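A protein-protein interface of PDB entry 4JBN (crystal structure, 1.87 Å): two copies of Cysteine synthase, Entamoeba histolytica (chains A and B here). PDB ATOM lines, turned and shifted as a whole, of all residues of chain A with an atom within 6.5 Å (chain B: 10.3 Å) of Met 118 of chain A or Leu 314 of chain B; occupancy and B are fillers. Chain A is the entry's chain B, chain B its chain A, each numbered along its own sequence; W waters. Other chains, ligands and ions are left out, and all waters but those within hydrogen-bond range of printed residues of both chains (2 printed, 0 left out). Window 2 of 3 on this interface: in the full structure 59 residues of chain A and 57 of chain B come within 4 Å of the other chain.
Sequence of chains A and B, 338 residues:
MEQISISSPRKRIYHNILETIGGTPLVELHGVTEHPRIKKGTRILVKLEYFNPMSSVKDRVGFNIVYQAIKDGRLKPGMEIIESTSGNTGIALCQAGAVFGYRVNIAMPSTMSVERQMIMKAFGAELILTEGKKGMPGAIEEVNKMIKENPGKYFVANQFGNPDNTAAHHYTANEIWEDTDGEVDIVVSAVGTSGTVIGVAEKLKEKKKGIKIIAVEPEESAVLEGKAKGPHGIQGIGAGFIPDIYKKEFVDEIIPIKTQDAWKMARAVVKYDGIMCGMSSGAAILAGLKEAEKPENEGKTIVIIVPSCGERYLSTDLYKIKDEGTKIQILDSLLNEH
Leu 314 of chain B touches Glu 115 of chain A (CD1 to O, 3.8 Å).
Leu 314 of chain B touches Met 118 of chain A.
CD1 of Ile 119 of chain A touches OE2 of Glu 311 of chain B, 3.9 Å away.
O of Ala 122 of chain A touches CG1 of Val 270 of chain B, at 3.5 Å.
N of Lys 271 of chain B touches O of Ala 122 of chain A, 3.9 Å away.
Ala 122 of chain A touches Tyr 319 of chain B (CB to CD1, 3.6 Å).
Val 270 of chain B touches Phe 123 of chain A.
Hydrophobic or aromatic side chains of chain A that line the printed part of chain B: Met 118, Ile 119, Ala 122 and Phe 123.
Along chain A the printed residues that touch a printed residue of chain B span positions 115 to 123.
Printed residues of chain B that touch a printed residue of chain A: Val 270, Lys 271, Glu 311, Leu 314 and Tyr 319.
Among the printed residues, no Asp or Glu carboxylate lies within 4 Å of a Lys or Arg side-chain nitrogen of the other chain.
Positions printed for both chains: 115 and 116.
Water W2 bridges O of Ala 122 of chain A (2.6 Å) and O of Arg 267 of chain B (2.9 Å).
Water W1 lies within hydrogen-bond range of O of Phe 123 of chain A and O of Lys 271 of chain B.
The side-chain sulfur of Met 276 of chain B lies within hydrogen-bond range of the backbone NH of Glu 311 of chain B (3.8 Å).
SG of Cys 309 of chain B lies close to N of Glu 311 of chain B.
Of the printed residues of chain B, Glu 115 of chain A touches Leu 314 (3.8 Å).
Leu 127 of chain A touches none of the printed residues of chain B.
Arg 312 of chain B touches none of the printed residues of chain A.
Printed residues of chain A within 4 Å of Tyr 319 of chain B: Ala 122 (3.6 Å).
The nearest printed residue of chain A that does not touch Leu 314 of chain B is Ile 119 of chain A (4.002 Å).
The nearest printed residue of chain B that does not touch Glu 115 of chain A is Glu 311 of chain B (6.4 Å).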
ATOM      1  N   SER A 113       2.244 -24.922  20.171  1.00  0.00           N
ATOM      2  CA  SER A 113       3.360 -24.352  20.936  1.00  0.00           C
ATOM      3  C   SER A 113       4.489 -23.726  20.089  1.00  0.00           C
ATOM      4  O   SER A 113       5.644 -24.209  20.079  1.00  0.00           O
ATOM      5  CB  SER A 113       3.930 -25.393  21.905  1.00  0.00           C
ATOM      6  OG  SER A 113       3.048 -25.585  22.992  1.00  0.00           O
ATOM      7  N   VAL A 114       4.175 -22.636  19.411  1.00  0.00           N
ATOM      8  CA  VAL A 114       5.230 -21.951  18.627  1.00  0.00           C
ATOM      9  C   VAL A 114       6.359 -21.321  19.529  1.00  0.00           C
ATOM     10  O   VAL A 114       7.476 -20.981  19.048  1.00  0.00           O
ATOM     11  CB  VAL A 114       4.567 -20.894  17.743  1.00  0.00           C
ATOM     12  CG1 VAL A 114       3.343 -20.358  18.481  1.00  0.00           C
ATOM     13  CG2 VAL A 114       5.554 -19.801  17.309  1.00  0.00           C
ATOM     14  N   GLU A 115       6.044 -21.119  20.816  1.00  0.00           N
ATOM     15  CA  GLU A 115       7.051 -20.617  21.779  1.00  0.00           C
ATOM     16  C   GLU A 115       8.025 -21.770  21.879  1.00  0.00           C
ATOM     17  O   GLU A 115       9.226 -21.586  21.670  1.00  0.00           O
ATOM     18  CB  GLU A 115       6.468 -20.230  23.161  1.00  0.00           C
ATOM     19  CG  GLU A 115       4.975 -19.838  23.199  1.00  0.00           C
ATOM     20  CD  GLU A 115       4.109 -20.938  23.811  1.00  0.00           C
ATOM     21  OE1 GLU A 115       3.529 -20.689  24.881  1.00  0.00           O
ATOM     22  OE2 GLU A 115       4.031 -22.066  23.262  1.00  0.00           O
ATOM     23  N   ARG A 116       7.491 -22.981  22.103  1.00  0.00           N
ATOM     24  CA  ARG A 116       8.345 -24.184  22.212  1.00  0.00           C
ATOM     25  C   ARG A 116       9.119 -24.516  20.930  1.00  0.00           C
ATOM     26  O   ARG A 116      10.271 -24.941  21.026  1.00  0.00           O
ATOM     27  CB  ARG A 116       7.592 -25.409  22.741  1.00  0.00           C
ATOM     28  CG  ARG A 116       7.282 -25.356  24.229  1.00  0.00           C
ATOM     29  CD  ARG A 116       6.834 -26.749  24.637  1.00  0.00           C
ATOM     30  NE  ARG A 116       6.209 -26.793  25.944  1.00  0.00           N
ATOM     31  CZ  ARG A 116       4.939 -26.483  26.159  1.00  0.00           C
ATOM     32  NH1 ARG A 116       4.184 -26.107  25.139  1.00  0.00           N
ATOM     33  NH2 ARG A 116       4.431 -26.542  27.395  1.00  0.00           N
ATOM     34  N   GLN A 117       8.572 -24.240  19.761  1.00  0.00           N
ATOM     35  CA  GLN A 117       9.287 -24.397  18.486  1.00  0.00           C
ATOM     36  C   GLN A 117      10.532 -23.570  18.426  1.00  0.00           C
ATOM     37  O   GLN A 117      11.561 -23.992  17.989  1.00  0.00           O
ATOM     38  CB  GLN A 117       8.427 -23.970  17.300  1.00  0.00           C
ATOM     39  CG  GLN A 117       7.229 -24.856  17.023  1.00  0.00           C
ATOM     40  CD  GLN A 117       6.361 -24.368  15.896  1.00  0.00           C
ATOM     41  OE1 GLN A 117       6.809 -23.730  14.992  1.00  0.00           O
ATOM     42  NE2 GLN A 117       5.105 -24.659  15.987  1.00  0.00           N
ATOM     43  N   MET A 118      10.388 -22.342  18.849  1.00  0.00           N
ATOM     44  CA  MET A 118      11.488 -21.434  18.913  1.00  0.00           C
ATOM     45  C   MET A 118      12.558 -21.959  19.881  1.00  0.00           C
ATOM     46  O   MET A 118      13.700 -21.981  19.547  1.00  0.00           O
ATOM     47  CB  MET A 118      10.982 -20.051  19.356  1.00  0.00           C
ATOM     48  CG  MET A 118       9.885 -19.474  18.465  1.00  0.00           C
ATOM     49  SD  MET A 118       9.313 -17.816  18.890  1.00  0.00           S
ATOM     50  CE  MET A 118       8.123 -18.234  20.144  1.00  0.00           C
ATOM     51  N   ILE A 119      12.146 -22.363  21.071  1.00  0.00           N
ATOM     52  CA  ILE A 119      13.097 -22.956  22.043  1.00  0.00           C
ATOM     53  C   ILE A 119      13.897 -24.095  21.346  1.00  0.00           C
ATOM     54  O   ILE A 119      15.139 -24.124  21.360  1.00  0.00           O
ATOM     55  CB  ILE A 119      12.428 -23.459  23.348  1.00  0.00           C
ATOM     56  CG1 ILE A 119      11.871 -22.265  24.168  1.00  0.00           C
ATOM     57  CG2 ILE A 119      13.478 -24.238  24.145  1.00  0.00           C
ATOM     58  CD1 ILE A 119      10.952 -22.593  25.343  1.00  0.00           C
ATOM     59  N   MET A 120      13.168 -24.979  20.674  1.00  0.00           N
ATOM     60  CA  MET A 120      13.802 -26.136  20.034  1.00  0.00           C
ATOM     61  C   MET A 120      14.777 -25.846  18.894  1.00  0.00           C
ATOM     62  O   MET A 120      15.883 -26.397  18.858  1.00  0.00           O
ATOM     63  CB  MET A 120      12.753 -27.191  19.712  1.00  0.00           C
ATOM     64  CG  MET A 120      12.259 -27.851  21.000  1.00  0.00           C
ATOM     65  SD  MET A 120      11.023 -29.106  20.739  1.00  0.00           S
ATOM     66  CE  MET A 120       9.489 -28.233  20.516  1.00  0.00           C
ATOM     67  N   LYS A 121      14.393 -24.927  18.012  1.00  0.00           N
ATOM     68  CA  LYS A 121      15.252 -24.454  16.953  1.00  0.00           C
ATOM     69  C   LYS A 121      16.519 -23.854  17.534  1.00  0.00           C
ATOM     70  O   LYS A 121      17.560 -24.061  16.964  1.00  0.00           O
ATOM     71  CB  LYS A 121      14.565 -23.434  16.032  1.00  0.00           C
ATOM     72  CG  LYS A 121      14.225 -23.997  14.636  1.00  0.00           C
ATOM     73  CD  LYS A 121      13.066 -23.207  14.007  1.00  0.00           C
ATOM     74  CE  LYS A 121      13.171 -23.123  12.477  1.00  0.00           C
ATOM     75  NZ  LYS A 121      11.850 -22.658  11.956  1.00  0.00           N
ATOM     76  N   ALA A 122      16.429 -23.178  18.686  1.00  0.00           N
ATOM     77  CA  ALA A 122      17.634 -22.549  19.270  1.00  0.00           C
ATOM     78  C   ALA A 122      18.717 -23.596  19.618  1.00  0.00           C
ATOM     79  O   ALA A 122      19.953 -23.387  19.414  1.00  0.00           O
ATOM     80  CB  ALA A 122      17.241 -21.699  20.453  1.00  0.00           C
ATOM     81  N   PHE A 123      18.237 -24.770  20.049  1.00  0.00           N
ATOM     82  CA  PHE A 123      19.096 -25.888  20.391  1.00  0.00           C
ATOM     83  C   PHE A 123      19.613 -26.590  19.170  1.00  0.00           C
ATOM     84  O   PHE A 123      20.376 -27.560  19.294  1.00  0.00           O
ATOM     85  CB  PHE A 123      18.346 -26.896  21.316  1.00  0.00           C
ATOM     86  CG  PHE A 123      18.322 -26.485  22.778  1.00  0.00           C
ATOM     87  CD1 PHE A 123      19.331 -26.926  23.626  1.00  0.00           C
ATOM     88  CD2 PHE A 123      17.302 -25.705  23.309  1.00  0.00           C
ATOM     89  CE1 PHE A 123      19.345 -26.551  24.990  1.00  0.00           C
ATOM     90  CE2 PHE A 123      17.328 -25.343  24.650  1.00  0.00           C
ATOM     91  CZ  PHE A 123      18.361 -25.739  25.479  1.00  0.00           C
ATOM     92  N   LEU A 127      12.900 -29.211  13.023  1.00  0.00           N
ATOM     93  CA  LEU A 127      11.495 -29.289  13.285  1.00  0.00           C
ATOM     94  C   LEU A 127      10.700 -29.854  12.112  1.00  0.00           C
ATOM     95  O   LEU A 127      10.873 -29.464  11.017  1.00  0.00           O
ATOM     96  CB  LEU A 127      10.951 -27.936  13.657  1.00  0.00           C
ATOM     97  CG  LEU A 127      11.374 -27.327  14.977  1.00  0.00           C
ATOM     98  CD1 LEU A 127      10.679 -26.018  15.199  1.00  0.00           C
ATOM     99  CD2 LEU A 127      11.085 -28.269  16.104  1.00  0.00           C
ATOM    100  N   GLU B 115       4.423  -9.601  28.751  1.00  0.00           N
ATOM    101  CA  GLU B 115       4.542 -10.912  29.334  1.00  0.00           C
ATOM    102  C   GLU B 115       4.941 -10.660  30.759  1.00  0.00           C
ATOM    103  O   GLU B 115       4.385 -11.276  31.653  1.00  0.00           O
ATOM    104  CB  GLU B 115       5.599 -11.781  28.669  1.00  0.00           C
ATOM    105  CG  GLU B 115       5.032 -12.808  27.703  1.00  0.00           C
ATOM    106  CD  GLU B 115       5.093 -12.327  26.269  1.00  0.00           C
ATOM    107  OE1 GLU B 115       6.035 -12.736  25.537  1.00  0.00           O
ATOM    108  OE2 GLU B 115       4.213 -11.517  25.889  1.00  0.00           O
ATOM    109  N   ARG B 116       5.890  -9.751  30.989  1.00  0.00           N
ATOM    110  CA  ARG B 116       6.352  -9.562  32.350  1.00  0.00           C
ATOM    111  C   ARG B 116       5.251  -8.906  33.182  1.00  0.00           C
ATOM    112  O   ARG B 116       5.163  -9.167  34.377  1.00  0.00           O
ATOM    113  CB  ARG B 116       7.669  -8.789  32.439  1.00  0.00           C
ATOM    114  CG  ARG B 116       8.912  -9.589  32.084  1.00  0.00           C
ATOM    115  CD  ARG B 116      10.124  -8.921  32.753  1.00  0.00           C
ATOM    116  NE  ARG B 116      11.419  -9.524  32.397  1.00  0.00           N
ATOM    117  CZ  ARG B 116      12.144  -9.177  31.334  1.00  0.00           C
ATOM    118  NH1 ARG B 116      11.686  -8.229  30.514  1.00  0.00           N
ATOM    119  NH2 ARG B 116      13.321  -9.779  31.087  1.00  0.00           N
ATOM    120  N   GLN B 235      19.340  -6.467  26.566  1.00  0.00           N
ATOM    121  CA  GLN B 235      18.383  -6.375  27.657  1.00  0.00           C
ATOM    122  C   GLN B 235      19.004  -6.756  29.015  1.00  0.00           C
ATOM    123  O   GLN B 235      19.799  -7.717  29.111  1.00  0.00           O
ATOM    124  CB  GLN B 235      17.191  -7.273  27.371  1.00  0.00           C
ATOM    125  CG  GLN B 235      16.258  -6.596  26.371  1.00  0.00           C
ATOM    126  CD  GLN B 235      14.866  -7.271  26.276  1.00  0.00           C
ATOM    127  OE1 GLN B 235      14.420  -7.989  27.193  1.00  0.00           O
ATOM    128  NE2 GLN B 235      14.203  -7.056  25.152  1.00  0.00           N
ATOM    129  N   ARG B 267      23.404 -17.258  20.897  1.00  0.00           N
ATOM    130  CA  ARG B 267      22.974 -18.318  19.970  1.00  0.00           C
ATOM    131  C   ARG B 267      23.972 -19.514  19.915  1.00  0.00           C
ATOM    132  O   ARG B 267      23.569 -20.708  19.928  1.00  0.00           O
ATOM    133  CB  ARG B 267      22.754 -17.675  18.593  1.00  0.00           C
ATOM    134  CG  ARG B 267      21.418 -16.953  18.486  1.00  0.00           C
ATOM    135  CD  ARG B 267      21.077 -16.649  16.974  1.00  0.00           C
ATOM    136  NE  ARG B 267      22.069 -15.771  16.329  1.00  0.00           N
ATOM    137  CZ  ARG B 267      22.063 -14.416  16.337  1.00  0.00           C
ATOM    138  NH1 ARG B 267      21.129 -13.729  17.013  1.00  0.00           N
ATOM    139  NH2 ARG B 267      23.010 -13.731  15.661  1.00  0.00           N
ATOM    140  N   VAL B 270      23.870 -21.765  23.277  1.00  0.00           N
ATOM    141  CA  VAL B 270      22.781 -22.832  23.376  1.00  0.00           C
ATOM    142  C   VAL B 270      22.991 -23.947  22.331  1.00  0.00           C
ATOM    143  O   VAL B 270      22.810 -25.165  22.620  1.00  0.00           O
ATOM    144  CB  VAL B 270      21.367 -22.215  23.345  1.00  0.00           C
ATOM    145  CG1 VAL B 270      21.126 -21.387  22.080  1.00  0.00           C
ATOM    146  CG2 VAL B 270      20.258 -23.259  23.647  1.00  0.00           C
ATOM    147  N   LYS B 271      23.463 -23.545  21.162  1.00  0.00           N
ATOM    148  CA  LYS B 271      23.745 -24.550  20.099  1.00  0.00           C
ATOM    149  C   LYS B 271      24.902 -25.522  20.452  1.00  0.00           C
ATOM    150  O   LYS B 271      24.728 -26.752  20.315  1.00  0.00           O
ATOM    151  CB  LYS B 271      23.970 -23.910  18.741  1.00  0.00           C
ATOM    152  CG  LYS B 271      24.152 -24.948  17.616  1.00  0.00           C
ATOM    153  CD  LYS B 271      23.677 -24.419  16.271  1.00  0.00           C
ATOM    154  CE  LYS B 271      23.584 -25.634  15.329  1.00  0.00           C
ATOM    155  NZ  LYS B 271      23.660 -25.290  13.891  1.00  0.00           N
ATOM    156  N   MET B 276      20.946 -22.553  27.578  1.00  0.00           N
ATOM    157  CA  MET B 276      20.102 -21.487  27.001  1.00  0.00           C
ATOM    158  C   MET B 276      20.174 -20.109  27.705  1.00  0.00           C
ATOM    159  O   MET B 276      19.192 -19.664  28.378  1.00  0.00           O
ATOM    160  CB  MET B 276      18.630 -21.879  26.944  1.00  0.00           C
ATOM    161  CG  MET B 276      17.896 -20.953  25.905  1.00  0.00           C
ATOM    162  SD  MET B 276      16.133 -21.408  25.997  1.00  0.00           S
ATOM    163  CE  MET B 276      15.601 -20.681  24.457  1.00  0.00           C
ATOM    164  N   CYS B 277      21.265 -19.408  27.502  1.00  0.00           N
ATOM    165  CA  CYS B 277      21.471 -18.197  28.186  1.00  0.00           C
ATOM    166  C   CYS B 277      20.833 -17.020  27.448  1.00  0.00           C
ATOM    167  O   CYS B 277      20.597 -17.061  26.229  1.00  0.00           O
ATOM    168  CB  CYS B 277      22.967 -17.970  28.354  1.00  0.00           C
ATOM    169  SG  CYS B 277      23.817 -17.667  26.768  1.00  0.00           S
ATOM    170  N   GLY B 278      20.585 -15.952  28.206  1.00  0.00           N
ATOM    171  CA  GLY B 278      19.961 -14.696  27.659  1.00  0.00           C
ATOM    172  C   GLY B 278      21.030 -13.777  27.078  1.00  0.00           C
ATOM    173  O   GLY B 278      22.186 -14.143  26.897  1.00  0.00           O
ATOM    174  N   MET B 279      20.601 -12.571  26.698  1.00  0.00           N
ATOM    175  CA  MET B 279      21.389 -11.681  25.852  1.00  0.00           C
ATOM    176  C   MET B 279      22.608 -11.115  26.625  1.00  0.00           C
ATOM    177  O   MET B 279      23.727 -11.107  26.138  1.00  0.00           O
ATOM    178  CB  MET B 279      20.508 -10.455  25.514  1.00  0.00           C
ATOM    179  CG  MET B 279      19.274 -10.787  24.719  1.00  0.00           C
ATOM    180  SD  MET B 279      18.291  -9.252  24.468  1.00  0.00           S
ATOM    181  CE  MET B 279      17.278  -9.787  23.065  1.00  0.00           C
ATOM    182  N   SER B 308      20.420 -14.745  33.214  1.00  0.00           N
ATOM    183  CA  SER B 308      19.031 -15.091  32.846  1.00  0.00           C
ATOM    184  C   SER B 308      19.059 -16.129  31.732  1.00  0.00           C
ATOM    185  O   SER B 308      20.152 -16.360  31.182  1.00  0.00           O
ATOM    186  CB  SER B 308      18.258 -13.862  32.344  1.00  0.00           C
ATOM    187  OG  SER B 308      18.817 -13.355  31.138  1.00  0.00           O
ATOM    188  N   CYS B 309      17.864 -16.725  31.427  1.00  0.00           N
ATOM    189  CA  CYS B 309      17.704 -17.834  30.461  1.00  0.00           C
ATOM    190  C   CYS B 309      17.115 -17.217  29.153  1.00  0.00           C
ATOM    191  O   CYS B 309      16.330 -16.291  29.213  1.00  0.00           O
ATOM    192  CB  CYS B 309      16.635 -18.883  31.058  1.00  0.00           C
ATOM    193  SG  CYS B 309      16.173 -20.244  29.973  1.00  0.00           S
ATOM    194  N   GLY B 310      17.494 -17.717  27.967  1.00  0.00           N
ATOM    195  CA  GLY B 310      16.818 -17.330  26.742  1.00  0.00           C
ATOM    196  C   GLY B 310      15.288 -17.415  26.635  1.00  0.00           C
ATOM    197  O   GLY B 310      14.713 -16.748  25.781  1.00  0.00           O
ATOM    198  N   GLU B 311      14.614 -18.250  27.437  1.00  0.00           N
ATOM    199  CA  GLU B 311      13.129 -18.335  27.364  1.00  0.00           C
ATOM    200  C   GLU B 311      12.378 -16.993  27.629  1.00  0.00           C
ATOM    201  O   GLU B 311      11.251 -16.716  27.116  1.00  0.00           O
ATOM    202  CB  GLU B 311      12.594 -19.426  28.282  1.00  0.00           C
ATOM    203  CG  GLU B 311      11.053 -19.576  28.278  1.00  0.00           C
ATOM    204  CD  GLU B 311      10.636 -20.870  28.949  1.00  0.00           C
ATOM    205  OE1 GLU B 311      11.481 -21.445  29.693  1.00  0.00           O
ATOM    206  OE2 GLU B 311       9.508 -21.328  28.701  1.00  0.00           O
ATOM    207  N   ARG B 312      13.009 -16.150  28.409  1.00  0.00           N
ATOM    208  CA  ARG B 312      12.409 -14.859  28.715  1.00  0.00           C
ATOM    209  C   ARG B 312      12.581 -13.853  27.512  1.00  0.00           C
ATOM    210  O   ARG B 312      12.086 -12.726  27.566  1.00  0.00           O
ATOM    211  CB  ARG B 312      12.991 -14.380  30.070  1.00  0.00           C
ATOM    212  CG  ARG B 312      12.189 -13.223  30.686  1.00  0.00           C
ATOM    213  CD  ARG B 312      12.440 -13.058  32.185  1.00  0.00           C
ATOM    214  NE  ARG B 312      11.745 -14.102  32.939  1.00  0.00           N
ATOM    215  CZ  ARG B 312      12.033 -14.451  34.188  1.00  0.00           C
ATOM    216  NH1 ARG B 312      13.036 -13.836  34.854  1.00  0.00           N
ATOM    217  NH2 ARG B 312      11.367 -15.457  34.751  1.00  0.00           N
ATOM    218  N   TYR B 313      13.204 -14.293  26.393  1.00  0.00           N
ATOM    219  CA  TYR B 313      13.548 -13.432  25.230  1.00  0.00           C
ATOM    220  C   TYR B 313      12.903 -13.885  23.889  1.00  0.00           C
ATOM    221  O   TYR B 313      13.293 -13.454  22.820  1.00  0.00           O
ATOM    222  CB  TYR B 313      15.076 -13.325  25.037  1.00  0.00           C
ATOM    223  CG  TYR B 313      15.772 -12.854  26.307  1.00  0.00           C
ATOM    224  CD1 TYR B 313      16.129 -11.505  26.469  1.00  0.00           C
ATOM    225  CD2 TYR B 313      16.024 -13.751  27.389  1.00  0.00           C
ATOM    226  CE1 TYR B 313      16.690 -11.034  27.671  1.00  0.00           C
ATOM    227  CE2 TYR B 313      16.652 -13.309  28.570  1.00  0.00           C
ATOM    228  CZ  TYR B 313      16.945 -11.950  28.719  1.00  0.00           C
ATOM    229  OH  TYR B 313      17.499 -11.507  29.886  1.00  0.00           O
ATOM    230  N   LEU B 314      11.943 -14.786  23.969  1.00  0.00           N
ATOM    231  CA  LEU B 314      11.366 -15.409  22.745  1.00  0.00           C
ATOM    232  C   LEU B 314      10.594 -14.379  21.863  1.00  0.00           C
ATOM    233  O   LEU B 314      10.490 -14.549  20.640  1.00  0.00           O
ATOM    234  CB  LEU B 314      10.424 -16.538  23.156  1.00  0.00           C
ATOM    235  CG  LEU B 314      11.079 -17.765  23.826  1.00  0.00           C
ATOM    236  CD1 LEU B 314       9.951 -18.734  24.088  1.00  0.00           C
ATOM    237  CD2 LEU B 314      12.205 -18.445  23.023  1.00  0.00           C
ATOM    238  N   SER B 315      10.058 -13.326  22.489  1.00  0.00           N
ATOM    239  CA  SER B 315       9.374 -12.257  21.720  1.00  0.00           C
ATOM    240  C   SER B 315      10.345 -11.194  21.186  1.00  0.00           C
ATOM    241  O   SER B 315       9.914 -10.262  20.498  1.00  0.00           O
ATOM    242  CB  SER B 315       8.325 -11.563  22.582  1.00  0.00           C
ATOM    243  OG  SER B 315       9.004 -10.871  23.641  1.00  0.00           O
ATOM    244  N   THR B 316      11.636 -11.315  21.529  1.00  0.00           N
ATOM    245  CA  THR B 316      12.694 -10.446  20.989  1.00  0.00           C
ATOM    246  C   THR B 316      13.277 -11.018  19.707  1.00  0.00           C
ATOM    247  O   THR B 316      12.840 -12.076  19.222  1.00  0.00           O
ATOM    248  CB  THR B 316      13.864 -10.211  22.006  1.00  0.00           C
ATOM    249  OG1 THR B 316      14.669 -11.414  22.107  1.00  0.00           O
ATOM    250  CG2 THR B 316      13.332  -9.814  23.367  1.00  0.00           C
ATOM    251  N   ASP B 317      14.297 -10.324  19.194  1.00  0.00           N
ATOM    252  CA  ASP B 317      15.073 -10.707  17.986  1.00  0.00           C
ATOM    253  C   ASP B 317      16.225 -11.732  18.230  1.00  0.00           C
ATOM    254  O   ASP B 317      16.843 -12.216  17.269  1.00  0.00           O
ATOM    255  CB  ASP B 317      15.657  -9.419  17.326  1.00  0.00           C
ATOM    256  CG  ASP B 317      14.583  -8.574  16.576  1.00  0.00           C
ATOM    257  OD1 ASP B 317      13.475  -9.086  16.300  1.00  0.00           O
ATOM    258  OD2 ASP B 317      14.861  -7.396  16.252  1.00  0.00           O
ATOM    259  N   LEU B 318      16.499 -12.047  19.508  1.00  0.00           N
ATOM    260  CA  LEU B 318      17.597 -12.982  19.927  1.00  0.00           C
ATOM    261  C   LEU B 318      17.790 -14.186  18.987  1.00  0.00           C
ATOM    262  O   LEU B 318      18.879 -14.373  18.437  1.00  0.00           O
ATOM    263  CB  LEU B 318      17.343 -13.469  21.371  1.00  0.00           C
ATOM    264  CG  LEU B 318      18.431 -14.356  22.009  1.00  0.00           C
ATOM    265  CD1 LEU B 318      19.830 -13.894  21.587  1.00  0.00           C
ATOM    266  CD2 LEU B 318      18.238 -14.515  23.530  1.00  0.00           C
ATOM    267  N   TYR B 319      16.718 -14.972  18.781  1.00  0.00           N
ATOM    268  CA  TYR B 319      16.812 -16.223  17.987  1.00  0.00           C
ATOM    269  C   TYR B 319      16.336 -16.102  16.558  1.00  0.00           C
ATOM    270  O   TYR B 319      16.304 -17.114  15.848  1.00  0.00           O
ATOM    271  CB  TYR B 319      16.057 -17.402  18.646  1.00  0.00           C
ATOM    272  CG  TYR B 319      16.609 -17.655  20.057  1.00  0.00           C
ATOM    273  CD1 TYR B 319      17.932 -18.128  20.232  1.00  0.00           C
ATOM    274  CD2 TYR B 319      15.848 -17.369  21.183  1.00  0.00           C
ATOM    275  CE1 TYR B 319      18.478 -18.317  21.495  1.00  0.00           C
ATOM    276  CE2 TYR B 319      16.380 -17.584  22.473  1.00  0.00           C
ATOM    277  CZ  TYR B 319      17.671 -18.053  22.603  1.00  0.00           C
ATOM    278  OH  TYR B 319      18.193 -18.267  23.846  1.00  0.00           O
ATOM    279  N   LYS B 320      15.948 -14.898  16.162  1.00  0.00           N
ATOM    280  CA  LYS B 320      15.285 -14.734  14.867  1.00  0.00           C
ATOM    281  C   LYS B 320      16.291 -14.573  13.699  1.00  0.00           C
ATOM    282  O   LYS B 320      15.983 -14.910  12.555  1.00  0.00           O
ATOM    283  CB  LYS B 320      14.132 -13.711  14.976  1.00  0.00           C
ATOM    284  CG  LYS B 320      13.110 -14.163  16.054  1.00  0.00           C
ATOM    285  CD  LYS B 320      11.744 -13.504  15.990  1.00  0.00           C
ATOM    286  CE  LYS B 320      11.890 -11.990  15.984  1.00  0.00           C
ATOM    287  NZ  LYS B 320      10.570 -11.315  16.116  1.00  0.00           N
ATOM    288  N   ILE B 321      17.500 -14.121  14.026  1.00  0.00           N
ATOM    289  CA  ILE B 321      18.639 -14.004  13.097  1.00  0.00           C
ATOM    290  C   ILE B 321      19.351 -15.359  12.958  1.00  0.00           C
ATOM    291  O   ILE B 321      19.777 -15.944  13.947  1.00  0.00           O
ATOM    292  CB  ILE B 321      19.631 -12.883  13.577  1.00  0.00           C
ATOM    293  CG1 ILE B 321      18.893 -11.533  13.777  1.00  0.00           C
ATOM    294  CG2 ILE B 321      20.832 -12.730  12.642  1.00  0.00           C
ATOM    295  CD1 ILE B 321      19.484 -10.602  14.824  1.00  0.00           C
HETATM  296  O   HOH W   1      22.956 -28.475  19.027  1.00  0.00           O
HETATM  297  O   HOH W   2      20.916 -21.085  18.768  1.00  0.00           O
